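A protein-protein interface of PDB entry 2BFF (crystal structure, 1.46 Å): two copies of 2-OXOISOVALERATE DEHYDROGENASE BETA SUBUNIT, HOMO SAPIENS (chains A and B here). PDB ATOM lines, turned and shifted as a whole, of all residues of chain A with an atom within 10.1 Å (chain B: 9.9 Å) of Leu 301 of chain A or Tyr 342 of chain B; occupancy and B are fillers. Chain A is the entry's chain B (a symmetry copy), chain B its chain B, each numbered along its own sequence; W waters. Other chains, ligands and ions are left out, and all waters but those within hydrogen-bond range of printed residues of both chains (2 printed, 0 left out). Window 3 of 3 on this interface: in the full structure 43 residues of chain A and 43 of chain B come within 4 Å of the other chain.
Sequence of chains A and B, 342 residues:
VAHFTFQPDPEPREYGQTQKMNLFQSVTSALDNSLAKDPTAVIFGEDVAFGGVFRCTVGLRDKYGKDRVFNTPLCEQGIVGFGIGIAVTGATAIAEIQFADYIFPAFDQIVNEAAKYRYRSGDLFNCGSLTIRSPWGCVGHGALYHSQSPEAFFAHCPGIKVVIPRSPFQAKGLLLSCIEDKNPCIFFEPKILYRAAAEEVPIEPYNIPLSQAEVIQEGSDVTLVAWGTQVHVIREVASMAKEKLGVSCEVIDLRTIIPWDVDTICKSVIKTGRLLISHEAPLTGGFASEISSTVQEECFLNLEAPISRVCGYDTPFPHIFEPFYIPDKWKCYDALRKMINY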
ATOM      1  N   VAL A 269      28.944 -34.746 -24.340  1.00  0.00           N
ATOM      2  CA  VAL A 269      28.531 -34.553 -22.947  1.00  0.00           C
ATOM      3  C   VAL A 269      27.244 -35.294 -22.638  1.00  0.00           C
ATOM      4  O   VAL A 269      27.034 -35.771 -21.505  1.00  0.00           O
ATOM      5  CB  VAL A 269      28.422 -33.061 -22.591  1.00  0.00           C
ATOM      6  CG1 VAL A 269      27.963 -32.889 -21.149  1.00  0.00           C
ATOM      7  CG2 VAL A 269      29.805 -32.410 -22.794  1.00  0.00           C
ATOM      8  N   ILE A 270      26.372 -35.437 -23.623  1.00  0.00           N
ATOM      9  CA  ILE A 270      25.164 -36.298 -23.370  1.00  0.00           C
ATOM     10  C   ILE A 270      25.596 -37.744 -23.062  1.00  0.00           C
ATOM     11  O   ILE A 270      25.009 -38.439 -22.173  1.00  0.00           O
ATOM     12  CB  ILE A 270      24.197 -36.249 -24.578  1.00  0.00           C
ATOM     13  CG1 ILE A 270      23.633 -34.817 -24.699  1.00  0.00           C
ATOM     14  CG2 ILE A 270      23.078 -37.370 -24.504  1.00  0.00           C
ATOM     15  CD1 ILE A 270      22.814 -34.515 -25.958  1.00  0.00           C
ATOM     16  N   LYS A 271      26.657 -38.220 -23.735  1.00  0.00           N
ATOM     17  CA  LYS A 271      27.170 -39.563 -23.484  1.00  0.00           C
ATOM     18  C   LYS A 271      27.885 -39.659 -22.126  1.00  0.00           C
ATOM     19  O   LYS A 271      27.704 -40.619 -21.363  1.00  0.00           O
ATOM     20  CB  LYS A 271      28.149 -39.986 -24.592  1.00  0.00           C
ATOM     21  CG  LYS A 271      28.894 -41.313 -24.250  1.00  0.00           C
ATOM     22  CD  LYS A 271      29.789 -41.802 -25.385  1.00  0.00           C
ATOM     23  CE  LYS A 271      30.994 -40.859 -25.610  1.00  0.00           C
ATOM     24  NZ  LYS A 271      31.873 -41.485 -26.615  1.00  0.00           N
ATOM     25  N   THR A 272      28.764 -38.696 -21.855  1.00  0.00           N
ATOM     26  CA  THR A 272      29.588 -38.846 -20.663  1.00  0.00           C
ATOM     27  C   THR A 272      28.991 -38.265 -19.383  1.00  0.00           C
ATOM     28  O   THR A 272      29.303 -38.774 -18.286  1.00  0.00           O
ATOM     29  CB  THR A 272      30.966 -38.153 -20.857  1.00  0.00           C
ATOM     30  OG1 THR A 272      30.736 -36.742 -21.000  1.00  0.00           O
ATOM     31  CG2 THR A 272      31.642 -38.629 -22.158  1.00  0.00           C
ATOM     32  N   GLY A 273      28.223 -37.183 -19.500  1.00  0.00           N
ATOM     33  CA  GLY A 273      27.642 -36.537 -18.326  1.00  0.00           C
ATOM     34  C   GLY A 273      28.536 -35.587 -17.542  1.00  0.00           C
ATOM     35  O   GLY A 273      28.105 -35.012 -16.539  1.00  0.00           O
ATOM     36  N   ARG A 274      29.757 -35.387 -18.043  1.00  0.00           N
ATOM     37  CA  ARG A 274      30.737 -34.528 -17.389  1.00  0.00           C
ATOM     38  C   ARG A 274      31.534 -33.758 -18.428  1.00  0.00           C
ATOM     39  O   ARG A 274      31.798 -34.267 -19.518  1.00  0.00           O
ATOM     40  CB  ARG A 274      31.687 -35.377 -16.513  1.00  0.00           C
ATOM     41  CG  ARG A 274      30.984 -36.269 -15.492  1.00  0.00           C
ATOM     42  CD  ARG A 274      31.938 -37.063 -14.607  1.00  0.00           C
ATOM     43  NE  ARG A 274      31.185 -37.912 -13.690  1.00  0.00           N
ATOM     44  CZ  ARG A 274      30.635 -39.088 -14.022  1.00  0.00           C
ATOM     45  NH1 ARG A 274      30.779 -39.569 -15.250  1.00  0.00           N
ATOM     46  NH2 ARG A 274      29.918 -39.769 -13.122  1.00  0.00           N
ATOM     47  N   THR A 294      26.428 -22.925 -22.826  1.00  0.00           N
ATOM     48  CA  THR A 294      25.664 -23.570 -23.905  1.00  0.00           C
ATOM     49  C   THR A 294      25.435 -25.070 -23.628  1.00  0.00           C
ATOM     50  O   THR A 294      24.307 -25.574 -23.834  1.00  0.00           O
ATOM     51  CB  THR A 294      26.413 -23.402 -25.223  1.00  0.00           C
ATOM     52  OG1 THR A 294      26.468 -21.985 -25.530  1.00  0.00           O
ATOM     53  CG2 THR A 294      25.673 -24.108 -26.370  1.00  0.00           C
ATOM     54  N   VAL A 295      26.484 -25.789 -23.215  1.00  0.00           N
ATOM     55  CA  VAL A 295      26.330 -27.181 -22.836  1.00  0.00           C
ATOM     56  C   VAL A 295      25.348 -27.327 -21.705  1.00  0.00           C
ATOM     57  O   VAL A 295      24.527 -28.262 -21.686  1.00  0.00           O
ATOM     58  CB  VAL A 295      27.680 -27.804 -22.478  1.00  0.00           C
ATOM     59  CG1 VAL A 295      27.538 -29.219 -21.886  1.00  0.00           C
ATOM     60  CG2 VAL A 295      28.544 -27.872 -23.752  1.00  0.00           C
ATOM     61  N   GLN A 296      25.413 -26.425 -20.728  1.00  0.00           N
ATOM     62  CA  GLN A 296      24.434 -26.476 -19.640  1.00  0.00           C
ATOM     63  C   GLN A 296      22.996 -26.382 -20.180  1.00  0.00           C
ATOM     64  O   GLN A 296      22.090 -27.126 -19.746  1.00  0.00           O
ATOM     65  CB  GLN A 296      24.702 -25.331 -18.665  1.00  0.00           C
ATOM     66  CG  GLN A 296      23.792 -25.346 -17.443  1.00  0.00           C
ATOM     67  CD  GLN A 296      22.667 -24.335 -17.486  1.00  0.00           C
ATOM     68  OE1 GLN A 296      21.780 -24.383 -16.632  1.00  0.00           O
ATOM     69  NE2 GLN A 296      22.704 -23.401 -18.453  1.00  0.00           N
ATOM     70  N   GLU A 297      22.779 -25.476 -21.134  1.00  0.00           N
ATOM     71  CA  GLU A 297      21.404 -25.250 -21.651  1.00  0.00           C
ATOM     72  C   GLU A 297      20.930 -26.521 -22.405  1.00  0.00           C
ATOM     73  O   GLU A 297      19.721 -26.897 -22.320  1.00  0.00           O
ATOM     74  CB  GLU A 297      21.434 -24.053 -22.604  1.00  0.00           C
ATOM     75  CG  GLU A 297      21.592 -22.705 -21.887  1.00  0.00           C
ATOM     76  CD  GLU A 297      22.211 -21.589 -22.757  1.00  0.00           C
ATOM     77  OE1 GLU A 297      22.571 -21.826 -23.940  1.00  0.00           O
ATOM     78  OE2 GLU A 297      22.402 -20.460 -22.243  1.00  0.00           O
ATOM     79  N   GLU A 298      21.826 -27.155 -23.164  1.00  0.00           N
ATOM     80  CA  GLU A 298      21.425 -28.208 -24.088  1.00  0.00           C
ATOM     81  C   GLU A 298      21.487 -29.581 -23.430  1.00  0.00           C
ATOM     82  O   GLU A 298      20.777 -30.506 -23.859  1.00  0.00           O
ATOM     83  CB  GLU A 298      22.315 -28.212 -25.342  1.00  0.00           C
ATOM     84  CG  GLU A 298      22.213 -26.967 -26.238  1.00  0.00           C
ATOM     85  CD  GLU A 298      20.769 -26.739 -26.669  1.00  0.00           C
ATOM     86  OE1 GLU A 298      20.123 -27.764 -27.056  1.00  0.00           O
ATOM     87  OE2 GLU A 298      20.255 -25.588 -26.552  1.00  0.00           O
ATOM     88  N   CYS A 299      22.351 -29.727 -22.416  1.00  0.00           N
ATOM     89  CA  CYS A 299      22.621 -31.057 -21.792  1.00  0.00           C
ATOM     90  C   CYS A 299      22.280 -31.119 -20.307  1.00  0.00           C
ATOM     91  O   CYS A 299      22.720 -32.023 -19.598  1.00  0.00           O
ATOM     92  CB  CYS A 299      24.097 -31.413 -21.967  1.00  0.00           C
ATOM     93  SG  CYS A 299      24.644 -31.318 -23.696  1.00  0.00           S
ATOM     94  N   PHE A 300      21.487 -30.152 -19.852  1.00  0.00           N
ATOM     95  CA  PHE A 300      21.163 -29.992 -18.424  1.00  0.00           C
ATOM     96  C   PHE A 300      20.823 -31.289 -17.693  1.00  0.00           C
ATOM     97  O   PHE A 300      21.436 -31.559 -16.674  1.00  0.00           O
ATOM     98  CB  PHE A 300      19.971 -29.029 -18.297  1.00  0.00           C
ATOM     99  CG  PHE A 300      19.690 -28.587 -16.892  1.00  0.00           C
ATOM    100  CD1 PHE A 300      20.581 -27.739 -16.203  1.00  0.00           C
ATOM    101  CD2 PHE A 300      18.552 -29.038 -16.225  1.00  0.00           C
ATOM    102  CE1 PHE A 300      20.316 -27.312 -14.900  1.00  0.00           C
ATOM    103  CE2 PHE A 300      18.284 -28.618 -14.915  1.00  0.00           C
ATOM    104  CZ  PHE A 300      19.171 -27.767 -14.240  1.00  0.00           C
ATOM    105  N   LEU A 301      19.887 -32.047 -18.251  1.00  0.00           N
ATOM    106  CA  LEU A 301      19.414 -33.296 -17.629  1.00  0.00           C
ATOM    107  C   LEU A 301      20.475 -34.386 -17.585  1.00  0.00           C
ATOM    108  O   LEU A 301      20.293 -35.371 -16.877  1.00  0.00           O
ATOM    109  CB  LEU A 301      18.156 -33.825 -18.330  1.00  0.00           C
ATOM    110  CG  LEU A 301      16.933 -32.919 -18.138  1.00  0.00           C
ATOM    111  CD1 LEU A 301      15.732 -33.474 -18.818  1.00  0.00           C
ATOM    112  CD2 LEU A 301      16.598 -32.706 -16.666  1.00  0.00           C
ATOM    113  N   ASN A 302      21.577 -34.217 -18.319  1.00  0.00           N
ATOM    114  CA  ASN A 302      22.629 -35.246 -18.396  1.00  0.00           C
ATOM    115  C   ASN A 302      23.824 -34.976 -17.482  1.00  0.00           C
ATOM    116  O   ASN A 302      24.673 -35.866 -17.334  1.00  0.00           O
ATOM    117  CB  ASN A 302      23.194 -35.303 -19.810  1.00  0.00           C
ATOM    118  CG  ASN A 302      22.116 -35.350 -20.859  1.00  0.00           C
ATOM    119  OD1 ASN A 302      21.874 -34.356 -21.574  1.00  0.00           O
ATOM    120  ND2 ASN A 302      21.503 -36.497 -21.001  1.00  0.00           N
ATOM    121  N   LEU A 303      23.893 -33.772 -16.898  1.00  0.00           N
ATOM    122  CA  LEU A 303      25.051 -33.347 -16.124  1.00  0.00           C
ATOM    123  C   LEU A 303      25.138 -33.982 -14.765  1.00  0.00           C
ATOM    124  O   LEU A 303      24.245 -33.812 -13.932  1.00  0.00           O
ATOM    125  CB  LEU A 303      25.036 -31.823 -15.936  1.00  0.00           C
ATOM    126  CG  LEU A 303      25.402 -31.086 -17.216  1.00  0.00           C
ATOM    127  CD1 LEU A 303      25.309 -29.520 -16.985  1.00  0.00           C
ATOM    128  CD2 LEU A 303      26.796 -31.447 -17.769  1.00  0.00           C
ATOM    129  N   GLU A 304      26.210 -34.747 -14.542  1.00  0.00           N
ATOM    130  CA  GLU A 304      26.402 -35.442 -13.267  1.00  0.00           C
ATOM    131  C   GLU A 304      27.133 -34.586 -12.237  1.00  0.00           C
ATOM    132  O   GLU A 304      27.088 -34.887 -11.023  1.00  0.00           O
ATOM    133  CB  GLU A 304      27.215 -36.742 -13.465  1.00  0.00           C
ATOM    134  CG  GLU A 304      26.584 -37.734 -14.419  1.00  0.00           C
ATOM    135  CD  GLU A 304      25.652 -38.696 -13.744  1.00  0.00           C
ATOM    136  OE1 GLU A 304      25.498 -38.654 -12.493  1.00  0.00           O
ATOM    137  OE2 GLU A 304      25.078 -39.513 -14.486  1.00  0.00           O
ATOM    138  N   ALA A 305      27.850 -33.558 -12.725  1.00  0.00           N
ATOM    139  CA  ALA A 305      28.691 -32.737 -11.876  1.00  0.00           C
ATOM    140  C   ALA A 305      28.732 -31.394 -12.627  1.00  0.00           C
ATOM    141  O   ALA A 305      28.459 -31.371 -13.858  1.00  0.00           O
ATOM    142  CB  ALA A 305      30.085 -33.296 -11.784  1.00  0.00           C
ATOM    143  N   ILE A 307      30.026 -28.278 -14.738  1.00  0.00           N
ATOM    144  CA  ILE A 307      31.034 -28.138 -15.782  1.00  0.00           C
ATOM    145  C   ILE A 307      32.234 -27.362 -15.224  1.00  0.00           C
ATOM    146  O   ILE A 307      32.053 -26.305 -14.607  1.00  0.00           O
ATOM    147  CB  ILE A 307      30.421 -27.417 -16.988  1.00  0.00           C
ATOM    148  CG1 ILE A 307      29.296 -28.313 -17.561  1.00  0.00           C
ATOM    149  CG2 ILE A 307      31.489 -27.133 -18.033  1.00  0.00           C
ATOM    150  CD1 ILE A 307      28.477 -27.603 -18.679  1.00  0.00           C
ATOM    151  N   GLY B 273      16.473 -21.132  -7.127  1.00  0.00           N
ATOM    152  CA  GLY B 273      16.681 -22.315  -7.959  1.00  0.00           C
ATOM    153  C   GLY B 273      16.573 -22.132  -9.467  1.00  0.00           C
ATOM    154  O   GLY B 273      16.737 -23.092 -10.223  1.00  0.00           O
ATOM    155  N   ARG B 274      16.357 -20.884  -9.889  1.00  0.00           N
ATOM    156  CA  ARG B 274      16.200 -20.555 -11.301  1.00  0.00           C
ATOM    157  C   ARG B 274      16.863 -19.223 -11.605  1.00  0.00           C
ATOM    158  O   ARG B 274      16.870 -18.322 -10.765  1.00  0.00           O
ATOM    159  CB  ARG B 274      14.700 -20.500 -11.670  1.00  0.00           C
ATOM    160  CG  ARG B 274      13.910 -21.759 -11.319  1.00  0.00           C
ATOM    161  CD  ARG B 274      12.444 -21.703 -11.733  1.00  0.00           C
ATOM    162  NE  ARG B 274      11.760 -22.925 -11.327  1.00  0.00           N
ATOM    163  CZ  ARG B 274      11.321 -23.175 -10.086  1.00  0.00           C
ATOM    164  NH1 ARG B 274      11.473 -22.268  -9.130  1.00  0.00           N
ATOM    165  NH2 ARG B 274      10.751 -24.350  -9.800  1.00  0.00           N
ATOM    166  N   PHE B 300      25.105 -25.430  -8.520  1.00  0.00           N
ATOM    167  CA  PHE B 300      24.712 -26.623  -9.288  1.00  0.00           C
ATOM    168  C   PHE B 300      23.583 -27.443  -8.669  1.00  0.00           C
ATOM    169  O   PHE B 300      22.606 -27.698  -9.353  1.00  0.00           O
ATOM    170  CB  PHE B 300      25.944 -27.528  -9.453  1.00  0.00           C
ATOM    171  CG  PHE B 300      25.747 -28.658 -10.419  1.00  0.00           C
ATOM    172  CD1 PHE B 300      25.611 -28.419 -11.801  1.00  0.00           C
ATOM    173  CD2 PHE B 300      25.662 -29.971  -9.959  1.00  0.00           C
ATOM    174  CE1 PHE B 300      25.443 -29.469 -12.706  1.00  0.00           C
ATOM    175  CE2 PHE B 300      25.487 -31.028 -10.862  1.00  0.00           C
ATOM    176  CZ  PHE B 300      25.361 -30.784 -12.237  1.00  0.00           C
ATOM    177  N   LEU B 303      19.881 -25.871  -8.881  1.00  0.00           N
ATOM    178  CA  LEU B 303      19.262 -25.518 -10.152  1.00  0.00           C
ATOM    179  C   LEU B 303      18.116 -26.411 -10.536  1.00  0.00           C
ATOM    180  O   LEU B 303      18.287 -27.620 -10.706  1.00  0.00           O
ATOM    181  CB  LEU B 303      20.301 -25.567 -11.282  1.00  0.00           C
ATOM    182  CG  LEU B 303      21.263 -24.390 -11.224  1.00  0.00           C
ATOM    183  CD1 LEU B 303      22.351 -24.521 -12.370  1.00  0.00           C
ATOM    184  CD2 LEU B 303      20.574 -23.013 -11.319  1.00  0.00           C
ATOM    185  N   GLU B 304      16.924 -25.819 -10.649  1.00  0.00           N
ATOM    186  CA  GLU B 304      15.721 -26.581 -10.994  1.00  0.00           C
ATOM    187  C   GLU B 304      15.509 -26.689 -12.501  1.00  0.00           C
ATOM    188  O   GLU B 304      14.739 -27.560 -12.967  1.00  0.00           O
ATOM    189  CB  GLU B 304      14.460 -25.926 -10.384  1.00  0.00           C
ATOM    190  CG  GLU B 304      14.489 -25.803  -8.875  1.00  0.00           C
ATOM    191  CD  GLU B 304      13.922 -27.000  -8.171  1.00  0.00           C
ATOM    192  OE1 GLU B 304      13.442 -27.956  -8.839  1.00  0.00           O
ATOM    193  OE2 GLU B 304      13.951 -26.969  -6.929  1.00  0.00           O
ATOM    194  N   ALA B 305      16.141 -25.772 -13.254  1.00  0.00           N
ATOM    195  CA  ALA B 305      15.934 -25.680 -14.687  1.00  0.00           C
ATOM    196  C   ALA B 305      17.253 -25.063 -15.186  1.00  0.00           C
ATOM    197  O   ALA B 305      17.981 -24.430 -14.375  1.00  0.00           O
ATOM    198  CB  ALA B 305      14.796 -24.751 -15.015  1.00  0.00           C
ATOM    199  N   PRO B 306      17.579 -25.239 -16.478  1.00  0.00           N
ATOM    200  CA  PRO B 306      18.792 -24.644 -17.005  1.00  0.00           C
ATOM    201  C   PRO B 306      18.739 -23.114 -16.904  1.00  0.00           C
ATOM    202  O   PRO B 306      17.675 -22.497 -17.031  1.00  0.00           O
ATOM    203  CB  PRO B 306      18.811 -25.046 -18.501  1.00  0.00           C
ATOM    204  CG  PRO B 306      17.710 -25.893 -18.753  1.00  0.00           C
ATOM    205  CD  PRO B 306      16.832 -25.961 -17.520  1.00  0.00           C
ATOM    206  N   ILE B 307      19.897 -22.502 -16.699  1.00  0.00           N
ATOM    207  CA  ILE B 307      19.995 -21.048 -16.673  1.00  0.00           C
ATOM    208  C   ILE B 307      19.716 -20.497 -18.077  1.00  0.00           C
ATOM    209  O   ILE B 307      20.291 -20.985 -19.058  1.00  0.00           O
ATOM    210  CB  ILE B 307      21.391 -20.640 -16.187  1.00  0.00           C
ATOM    211  CG1 ILE B 307      21.553 -21.132 -14.729  1.00  0.00           C
ATOM    212  CG2 ILE B 307      21.566 -19.133 -16.286  1.00  0.00           C
ATOM    213  CD1 ILE B 307      23.000 -20.937 -14.188  1.00  0.00           C
ATOM    214  N   SER B 308      18.816 -19.522 -18.179  1.00  0.00           N
ATOM    215  CA  SER B 308      18.408 -19.007 -19.482  1.00  0.00           C
ATOM    216  C   SER B 308      19.112 -17.673 -19.745  1.00  0.00           C
ATOM    217  O   SER B 308      19.304 -16.879 -18.826  1.00  0.00           O
ATOM    218  CB  SER B 308      16.870 -18.863 -19.543  1.00  0.00           C
ATOM    219  OG  SER B 308      16.433 -17.832 -20.413  1.00  0.00           O
ATOM    220  N   ASP B 334       8.581 -14.933 -22.391  1.00  0.00           N
ATOM    221  CA  ASP B 334       8.395 -16.254 -22.998  1.00  0.00           C
ATOM    222  C   ASP B 334       9.455 -17.267 -22.546  1.00  0.00           C
ATOM    223  O   ASP B 334       9.149 -18.395 -22.224  1.00  0.00           O
ATOM    224  CB  ASP B 334       8.438 -16.167 -24.512  1.00  0.00           C
ATOM    225  CG  ASP B 334       7.919 -17.438 -25.154  1.00  0.00           C
ATOM    226  OD1 ASP B 334       6.777 -17.837 -24.853  1.00  0.00           O
ATOM    227  OD2 ASP B 334       8.621 -18.077 -25.970  1.00  0.00           O
ATOM    228  N   ALA B 335      10.705 -16.802 -22.462  1.00  0.00           N
ATOM    229  CA  ALA B 335      11.789 -17.622 -21.941  1.00  0.00           C
ATOM    230  C   ALA B 335      11.530 -17.985 -20.483  1.00  0.00           C
ATOM    231  O   ALA B 335      11.769 -19.132 -20.052  1.00  0.00           O
ATOM    232  CB  ALA B 335      13.143 -16.866 -22.079  1.00  0.00           C
ATOM    233  N   LEU B 336      11.066 -16.998 -19.708  1.00  0.00           N
ATOM    234  CA  LEU B 336      10.751 -17.260 -18.301  1.00  0.00           C
ATOM    235  C   LEU B 336       9.665 -18.316 -18.160  1.00  0.00           C
ATOM    236  O   LEU B 336       9.752 -19.189 -17.307  1.00  0.00           O
ATOM    237  CB  LEU B 336      10.276 -15.961 -17.639  1.00  0.00           C
ATOM    238  CG  LEU B 336       9.926 -15.998 -16.143  1.00  0.00           C
ATOM    239  CD1 LEU B 336      10.987 -16.758 -15.321  1.00  0.00           C
ATOM    240  CD2 LEU B 336       9.761 -14.555 -15.611  1.00  0.00           C
ATOM    241  N   ARG B 337       8.644 -18.217 -18.999  1.00  0.00           N
ATOM    242  CA  ARG B 337       7.497 -19.154 -18.955  1.00  0.00           C
ATOM    243  C   ARG B 337       7.989 -20.578 -19.205  1.00  0.00           C
ATOM    244  O   ARG B 337       7.626 -21.507 -18.459  1.00  0.00           O
ATOM    245  CB  ARG B 337       6.443 -18.724 -19.981  1.00  0.00           C
ATOM    246  CG  ARG B 337       5.071 -19.397 -19.918  1.00  0.00           C
ATOM    247  CD  ARG B 337       4.182 -19.098 -21.161  1.00  0.00           C
ATOM    248  NE  ARG B 337       4.968 -19.297 -22.389  1.00  0.00           N
ATOM    249  CZ  ARG B 337       5.200 -20.481 -22.986  1.00  0.00           C
ATOM    250  NH1 ARG B 337       4.665 -21.609 -22.505  1.00  0.00           N
ATOM    251  NH2 ARG B 337       5.963 -20.538 -24.075  1.00  0.00           N
ATOM    252  N   LYS B 338       8.819 -20.744 -20.233  1.00  0.00           N
ATOM    253  CA  LYS B 338       9.369 -22.050 -20.570  1.00  0.00           C
ATOM    254  C   LYS B 338      10.228 -22.577 -19.410  1.00  0.00           C
ATOM    255  O   LYS B 338      10.118 -23.743 -19.026  1.00  0.00           O
ATOM    256  CB  LYS B 338      10.179 -21.968 -21.860  1.00  0.00           C
ATOM    257  CG  LYS B 338       9.347 -21.726 -23.099  1.00  0.00           C
ATOM    258  CD  LYS B 338      10.348 -21.471 -24.193  1.00  0.00           C
ATOM    259  CE  LYS B 338       9.744 -21.224 -25.550  1.00  0.00           C
ATOM    260  NZ  LYS B 338      10.898 -20.933 -26.456  1.00  0.00           N
ATOM    261  N   MET B 339      11.052 -21.704 -18.824  1.00  0.00           N
ATOM    262  CA  MET B 339      11.914 -22.110 -17.725  1.00  0.00           C
ATOM    263  C   MET B 339      11.108 -22.568 -16.508  1.00  0.00           C
ATOM    264  O   MET B 339      11.443 -23.591 -15.912  1.00  0.00           O
ATOM    265  CB  MET B 339      12.906 -20.989 -17.366  1.00  0.00           C
ATOM    266  CG  MET B 339      14.082 -21.488 -16.518  1.00  0.00           C
ATOM    267  SD  MET B 339      15.316 -20.178 -16.205  1.00  0.00           S
ATOM    268  CE  MET B 339      14.281 -18.972 -15.468  1.00  0.00           C
ATOM    269  N   ILE B 340      10.046 -21.824 -16.164  1.00  0.00           N
ATOM    270  CA  ILE B 340       9.147 -22.148 -15.034  1.00  0.00           C
ATOM    271  C   ILE B 340       8.509 -23.530 -15.263  1.00  0.00           C
ATOM    272  O   ILE B 340       8.273 -24.271 -14.308  1.00  0.00           O
ATOM    273  CB  ILE B 340       8.052 -21.017 -14.814  1.00  0.00           C
ATOM    274  CG1 ILE B 340       8.666 -19.762 -14.181  1.00  0.00           C
ATOM    275  CG2 ILE B 340       6.876 -21.514 -13.989  1.00  0.00           C
ATOM    276  CD1 ILE B 340       9.325 -19.974 -12.803  1.00  0.00           C
ATOM    277  N   ASN B 341       8.263 -23.888 -16.521  1.00  0.00           N
ATOM    278  CA  ASN B 341       7.607 -25.157 -16.855  1.00  0.00           C
ATOM    279  C   ASN B 341       8.570 -26.310 -17.165  1.00  0.00           C
ATOM    280  O   ASN B 341       8.121 -27.419 -17.474  1.00  0.00           O
ATOM    281  CB  ASN B 341       6.675 -24.962 -18.050  1.00  0.00           C
ATOM    282  CG  ASN B 341       5.483 -24.101 -17.713  1.00  0.00           C
ATOM    283  OD1 ASN B 341       4.817 -24.304 -16.673  1.00  0.00           O
ATOM    284  ND2 ASN B 341       5.167 -23.170 -18.592  1.00  0.00           N
ATOM    285  N   TYR B 342       9.878 -26.058 -17.068  1.00  0.00           N
ATOM    286  CA  TYR B 342      10.913 -27.014 -17.513  1.00  0.00           C
ATOM    287  C   TYR B 342      10.772 -28.423 -16.962  1.00  0.00           C
ATOM    288  O   TYR B 342      10.700 -28.580 -15.727  1.00  0.00           O
ATOM    289  CB  TYR B 342      12.314 -26.503 -17.165  1.00  0.00           C
ATOM    290  CG  TYR B 342      13.416 -27.366 -17.720  1.00  0.00           C
ATOM    291  CD1 TYR B 342      14.009 -28.370 -16.942  1.00  0.00           C
ATOM    292  CD2 TYR B 342      13.872 -27.182 -19.018  1.00  0.00           C
ATOM    293  CE1 TYR B 342      15.056 -29.166 -17.452  1.00  0.00           C
ATOM    294  CE2 TYR B 342      14.906 -27.953 -19.541  1.00  0.00           C
ATOM    295  CZ  TYR B 342      15.480 -28.975 -18.757  1.00  0.00           C
ATOM    296  OH  TYR B 342      16.515 -29.735 -19.292  1.00  0.00           O
ATOM    297  OXT TYR B 342      10.766 -29.397 -17.752  1.00  0.00           O
HETATM  298  O   HOH W   1      18.074 -29.046 -21.610  1.00  0.00           O
HETATM  299  O   HOH W   2      22.891 -20.438 -19.633  1.00  0.00           O
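The backbone NH of Ile 307 of chain B lies within hydrogen-bond range of the side-chain amide oxygen of Gln 296 of chain A, at 2.7 Å.
Among the printed residues, merely in contact across the chains: Gln 296 of chain A with Pro 306 of chain B (3.0 Å), Glu 297 of chain A with Ile 307 of chain B (3.6 Å), Phe 300 of chain A with Leu 303 of chain B (3.6 Å), Phe 300 of chain A with Ala 305 of chain B (3.4 Å), Phe 300 of chain A with Pro 306 of chain B (3.7 Å), Phe 300 of chain A with Tyr 342 of chain B (3.7 Å), Leu 301 of chain A with Tyr 342 of chain B (3.4 Å), Leu 303 of chain A with Phe 300 of chain B (3.6 Å) and Ala 305 of chain A with Phe 300 of chain B (3.4 Å).
Phe 300 of chain A touches just these residues of chain B: Leu 303 (3.6 Å), Ala 305 (3.4 Å), Pro 306 (3.7 Å) and Tyr 342 (3.7 Å).
Leu 301 of chain A touches just one residue of chain B: Tyr 342 (3.4 Å).
Of the printed residues of chain B, Ala 305 of chain A touches Phe 300 (3.4 Å).
Printed residues of chain A within 4 Å of Phe 300 of chain B: Leu 303 and Ala 305.
Of the printed residues of chain A, Ala 305 of chain B touches Phe 300 (3.4 Å).
No residue of chain A comes within 4 Å of Asn 341 of chain B.
Tyr 342 of chain B touches just these residues of chain A: Phe 300 and Leu 301.
The nearest residue of chain B that does not touch Leu 301 of chain A is Pro 306 of chain B (6.5 Å).
Of the 19 printed residues of chain A, 6 touch a printed residue of chain B.
Hydrophobic or aromatic side chains of chain A that line the printed part of chain B: Phe 300, Leu 301 and Leu 303.
Among the printed residues, no Asp or Glu carboxylate lies within 4 Å of a Lys or Arg side-chain nitrogen of the other chain.
Phe 300 of chain A touches Leu 303 of chain B, and with the chains exchanged Leu 303 of chain A touches Phe 300 of chain B.
Phe 300 of chain A touches Ala 305 of chain B, and with the chains exchanged Ala 305 of chain A touches Phe 300 of chain B.
Positions printed for both chains: 273, 274, 300, 303, 304, 305 and 307.
Of the 10 pairs that touch across the chains among the printed residues, 4 have their exchanged pair printed and touching as well.
Water W2 lies within hydrogen-bond range of OE2 of Glu 297 of chain A (2.7 Å), O of Ile 307 of chain B (2.7 Å) and NE2 of Gln 296 of chain A (3.2 Å).
Water W1 bridges the backbone carbonyl oxygen (O) of Glu 297 of chain A and the side-chain hydroxyl (OH) of Tyr 342 of chain B.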
